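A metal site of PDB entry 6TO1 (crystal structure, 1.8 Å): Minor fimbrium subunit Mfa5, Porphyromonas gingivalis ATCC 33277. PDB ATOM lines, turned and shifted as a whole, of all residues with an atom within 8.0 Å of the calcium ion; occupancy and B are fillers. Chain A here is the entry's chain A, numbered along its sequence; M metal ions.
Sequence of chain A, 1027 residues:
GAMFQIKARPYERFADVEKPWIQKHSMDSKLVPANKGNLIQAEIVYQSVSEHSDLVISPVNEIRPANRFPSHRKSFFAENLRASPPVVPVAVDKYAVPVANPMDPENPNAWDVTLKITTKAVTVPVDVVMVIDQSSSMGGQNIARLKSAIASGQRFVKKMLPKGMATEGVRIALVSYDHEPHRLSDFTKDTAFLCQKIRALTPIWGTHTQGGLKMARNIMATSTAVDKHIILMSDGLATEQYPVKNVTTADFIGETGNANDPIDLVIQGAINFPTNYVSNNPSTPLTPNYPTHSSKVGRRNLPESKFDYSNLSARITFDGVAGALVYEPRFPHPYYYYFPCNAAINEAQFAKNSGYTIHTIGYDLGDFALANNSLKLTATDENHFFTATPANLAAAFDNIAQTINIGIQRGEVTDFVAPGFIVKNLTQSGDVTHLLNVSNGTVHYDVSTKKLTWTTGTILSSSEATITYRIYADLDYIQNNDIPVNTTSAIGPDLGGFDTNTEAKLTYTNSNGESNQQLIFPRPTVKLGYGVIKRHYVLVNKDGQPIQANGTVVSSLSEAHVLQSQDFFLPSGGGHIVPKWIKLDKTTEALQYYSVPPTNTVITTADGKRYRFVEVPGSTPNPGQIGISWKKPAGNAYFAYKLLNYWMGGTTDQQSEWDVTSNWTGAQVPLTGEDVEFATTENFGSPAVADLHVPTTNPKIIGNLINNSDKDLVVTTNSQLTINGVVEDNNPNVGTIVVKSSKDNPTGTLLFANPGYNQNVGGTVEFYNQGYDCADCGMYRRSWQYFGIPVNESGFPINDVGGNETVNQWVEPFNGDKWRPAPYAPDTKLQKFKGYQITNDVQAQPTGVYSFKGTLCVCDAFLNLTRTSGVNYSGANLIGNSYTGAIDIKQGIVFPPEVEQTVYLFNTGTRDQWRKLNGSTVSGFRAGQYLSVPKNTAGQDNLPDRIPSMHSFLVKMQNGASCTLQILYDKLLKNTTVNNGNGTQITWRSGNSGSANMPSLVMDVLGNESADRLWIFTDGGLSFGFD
Five residues have an atom within 4 Å of the calcium ion: Asn 280, Asn 281, Thr 284, Leu 286 and Asp 319.
The nearest printed residue that does not touch the calcium ion is Pro 285 (4.1 Å).
The calcium ion is bound by O of Asn 281 (2.2 Å), O of Leu 286 (2.2 Å), O of Thr 284 (2.4 Å), OG1 of Thr 284 (2.4 Å), OD2 of Asp 319 (2.6 Å) and OD1 of Asn 280 (2.8 Å).
The calcium ion has six donor atoms within binding distance.
N of Ser 283 is in hydrogen-bond range of OD1 of Asn 281, 3.0 Å away.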
ATOM      1  N   SER A 279      20.867  -2.421  14.441  1.00  0.00           N
ATOM      2  CA  SER A 279      22.040  -3.108  13.928  1.00  0.00           C
ATOM      3  C   SER A 279      22.726  -3.978  14.969  1.00  0.00           C
ATOM      4  O   SER A 279      23.327  -3.462  15.916  1.00  0.00           O
ATOM      5  CB  SER A 279      23.052  -2.093  13.400  1.00  0.00           C
ATOM      6  OG  SER A 279      23.458  -1.218  14.448  1.00  0.00           O
ATOM      7  N   ASN A 280      22.662  -5.298  14.768  1.00  0.00           N
ATOM      8  CA  ASN A 280      23.432  -6.225  15.577  1.00  0.00           C
ATOM      9  C   ASN A 280      23.642  -7.530  14.835  1.00  0.00           C
ATOM     10  O   ASN A 280      22.696  -8.062  14.253  1.00  0.00           O
ATOM     11  CB  ASN A 280      22.730  -6.517  16.881  1.00  0.00           C
ATOM     12  CG  ASN A 280      23.488  -7.555  17.714  1.00  0.00           C
ATOM     13  OD1 ASN A 280      24.697  -7.425  17.917  1.00  0.00           O
ATOM     14  ND2 ASN A 280      22.782  -8.606  18.145  1.00  0.00           N
ATOM     15  N   ASN A 281      24.881  -8.045  14.848  1.00  0.00           N
ATOM     16  CA  ASN A 281      25.158  -9.379  14.328  1.00  0.00           C
ATOM     17  C   ASN A 281      24.968 -10.378  15.452  1.00  0.00           C
ATOM     18  O   ASN A 281      25.796 -10.401  16.376  1.00  0.00           O
ATOM     19  CB  ASN A 281      26.568  -9.467  13.772  1.00  0.00           C
ATOM     20  CG  ASN A 281      26.826 -10.771  13.025  1.00  0.00           C
ATOM     21  OD1 ASN A 281      26.194 -11.794  13.292  1.00  0.00           O
ATOM     22  ND2 ASN A 281      27.735 -10.727  12.069  1.00  0.00           N
ATOM     23  N   PRO A 282      23.904 -11.181  15.460  1.00  0.00           N
ATOM     24  CA  PRO A 282      23.671 -12.064  16.618  1.00  0.00           C
ATOM     25  C   PRO A 282      24.767 -13.092  16.813  1.00  0.00           C
ATOM     26  O   PRO A 282      24.865 -13.658  17.917  1.00  0.00           O
ATOM     27  CB  PRO A 282      22.322 -12.728  16.291  1.00  0.00           C
ATOM     28  CG  PRO A 282      22.196 -12.653  14.807  1.00  0.00           C
ATOM     29  CD  PRO A 282      22.929 -11.401  14.377  1.00  0.00           C
ATOM     30  N   SER A 283      25.592 -13.326  15.798  1.00  0.00           N
ATOM     31  CA  SER A 283      26.650 -14.321  15.868  1.00  0.00           C
ATOM     32  C   SER A 283      27.894 -13.834  16.595  1.00  0.00           C
ATOM     33  O   SER A 283      28.686 -14.668  17.054  1.00  0.00           O
ATOM     34  CB  SER A 283      27.035 -14.753  14.454  1.00  0.00           C
ATOM     35  OG  SER A 283      25.978 -15.431  13.812  1.00  0.00           O
ATOM     36  N   THR A 284      28.077 -12.563  16.706  1.00  0.00           N
ATOM     37  CA  THR A 284      29.268 -12.017  17.353  1.00  0.00           C
ATOM     38  C   THR A 284      28.921 -11.510  18.743  1.00  0.00           C
ATOM     39  O   THR A 284      27.799 -11.065  18.991  1.00  0.00           O
ATOM     40  CB  THR A 284      29.829 -10.839  16.557  1.00  0.00           C
ATOM     41  OG1 THR A 284      28.911  -9.738  16.634  1.00  0.00           O
ATOM     42  CG2 THR A 284      30.025 -11.221  15.111  1.00  0.00           C
ATOM     43  N   PRO A 285      29.866 -11.566  19.688  1.00  0.00           N
ATOM     44  CA  PRO A 285      29.556 -11.089  21.041  1.00  0.00           C
ATOM     45  C   PRO A 285      29.342  -9.606  21.108  1.00  0.00           C
ATOM     46  O   PRO A 285      28.674  -9.142  22.034  1.00  0.00           O
ATOM     47  CB  PRO A 285      30.785 -11.504  21.861  1.00  0.00           C
ATOM     48  CG  PRO A 285      31.466 -12.554  21.067  1.00  0.00           C
ATOM     49  CD  PRO A 285      31.185 -12.233  19.618  1.00  0.00           C
ATOM     50  N   LEU A 286      29.891  -8.833  20.173  1.00  0.00           N
ATOM     51  CA  LEU A 286      29.725  -7.389  20.184  1.00  0.00           C
ATOM     52  C   LEU A 286      28.243  -7.044  20.104  1.00  0.00           C
ATOM     53  O   LEU A 286      27.483  -7.613  19.317  1.00  0.00           O
ATOM     54  CB  LEU A 286      30.500  -6.787  19.028  1.00  0.00           C
ATOM     55  CG  LEU A 286      30.361  -5.277  18.749  1.00  0.00           C
ATOM     56  CD1 LEU A 286      30.906  -4.447  19.910  1.00  0.00           C
ATOM     57  CD2 LEU A 286      31.056  -4.936  17.453  1.00  0.00           C
ATOM     58  N   THR A 287      27.806  -6.137  20.970  1.00  0.00           N
ATOM     59  CA  THR A 287      26.419  -5.705  20.910  1.00  0.00           C
ATOM     60  C   THR A 287      26.350  -4.195  20.990  1.00  0.00           C
ATOM     61  O   THR A 287      27.189  -3.546  21.626  1.00  0.00           O
ATOM     62  CB  THR A 287      25.581  -6.323  22.041  1.00  0.00           C
ATOM     63  OG1 THR A 287      26.126  -5.931  23.308  1.00  0.00           O
ATOM     64  CG2 THR A 287      25.602  -7.845  21.931  1.00  0.00           C
ATOM     65  N   PRO A 288      25.372  -3.609  20.314  1.00  0.00           N
ATOM     66  CA  PRO A 288      25.191  -2.158  20.419  1.00  0.00           C
ATOM     67  C   PRO A 288      24.586  -1.799  21.763  1.00  0.00           C
ATOM     68  O   PRO A 288      24.018  -2.631  22.452  1.00  0.00           O
ATOM     69  CB  PRO A 288      24.214  -1.849  19.271  1.00  0.00           C
ATOM     70  CG  PRO A 288      23.391  -3.094  19.175  1.00  0.00           C
ATOM     71  CD  PRO A 288      24.322  -4.256  19.498  1.00  0.00           C
ATOM     72  N   TYR A 290      21.391   0.054  23.202  1.00  0.00           N
ATOM     73  CA  TYR A 290      20.059   0.163  22.623  1.00  0.00           C
ATOM     74  C   TYR A 290      19.354   1.465  23.001  1.00  0.00           C
ATOM     75  O   TYR A 290      19.663   2.074  24.032  1.00  0.00           O
ATOM     76  CB  TYR A 290      19.224  -1.046  23.049  1.00  0.00           C
ATOM     77  CG  TYR A 290      19.653  -2.309  22.337  1.00  0.00           C
ATOM     78  CD1 TYR A 290      19.099  -2.664  21.108  1.00  0.00           C
ATOM     79  CD2 TYR A 290      20.629  -3.141  22.881  1.00  0.00           C
ATOM     80  CE1 TYR A 290      19.511  -3.804  20.439  1.00  0.00           C
ATOM     81  CE2 TYR A 290      21.025  -4.286  22.217  1.00  0.00           C
ATOM     82  CZ  TYR A 290      20.473  -4.613  21.005  1.00  0.00           C
ATOM     83  OH  TYR A 290      20.872  -5.735  20.336  1.00  0.00           O
ATOM     84  N   PHE A 318      27.371  -1.218  11.695  1.00  0.00           N
ATOM     85  CA  PHE A 318      27.898  -1.464  13.028  1.00  0.00           C
ATOM     86  C   PHE A 318      27.972  -2.976  13.154  1.00  0.00           C
ATOM     87  O   PHE A 318      26.991  -3.660  12.818  1.00  0.00           O
ATOM     88  CB  PHE A 318      26.999  -0.912  14.122  1.00  0.00           C
ATOM     89  CG  PHE A 318      27.448  -1.330  15.508  1.00  0.00           C
ATOM     90  CD1 PHE A 318      28.512  -0.696  16.099  1.00  0.00           C
ATOM     91  CD2 PHE A 318      26.827  -2.376  16.173  1.00  0.00           C
ATOM     92  CE1 PHE A 318      28.955  -1.071  17.353  1.00  0.00           C
ATOM     93  CE2 PHE A 318      27.262  -2.761  17.433  1.00  0.00           C
ATOM     94  CZ  PHE A 318      28.309  -2.101  18.013  1.00  0.00           C
ATOM     95  N   ASP A 319      29.098  -3.522  13.629  1.00  0.00           N
ATOM     96  CA  ASP A 319      29.184  -4.982  13.848  1.00  0.00           C
ATOM     97  C   ASP A 319      28.996  -5.743  12.532  1.00  0.00           C
ATOM     98  O   ASP A 319      28.449  -6.845  12.497  1.00  0.00           O
ATOM     99  CB  ASP A 319      28.154  -5.417  14.890  1.00  0.00           C
ATOM    100  CG  ASP A 319      28.400  -6.836  15.485  1.00  0.00           C
ATOM    101  OD1 ASP A 319      29.542  -7.325  15.470  1.00  0.00           O
ATOM    102  OD2 ASP A 319      27.433  -7.447  15.990  1.00  0.00           O
ATOM    103  N   GLY A 320      29.365  -5.087  11.434  1.00  0.00           N
ATOM    104  CA  GLY A 320      29.259  -5.620  10.100  1.00  0.00           C
ATOM    105  C   GLY A 320      27.879  -5.624   9.479  1.00  0.00           C
ATOM    106  O   GLY A 320      27.712  -6.192   8.398  1.00  0.00           O
ATOM    107  N   VAL A 321      26.866  -5.039  10.131  1.00  0.00           N
ATOM    108  CA  VAL A 321      25.499  -5.084   9.624  1.00  0.00           C
ATOM    109  C   VAL A 321      24.880  -3.686   9.741  1.00  0.00           C
ATOM    110  O   VAL A 321      25.429  -2.792  10.377  1.00  0.00           O
ATOM    111  CB  VAL A 321      24.610  -6.116  10.364  1.00  0.00           C
ATOM    112  CG1 VAL A 321      25.194  -7.537  10.231  1.00  0.00           C
ATOM    113  CG2 VAL A 321      24.427  -5.746  11.822  1.00  0.00           C
HETATM  114 CA    CA M   1      26.881  -9.164  17.823  1.00  0.00          CA
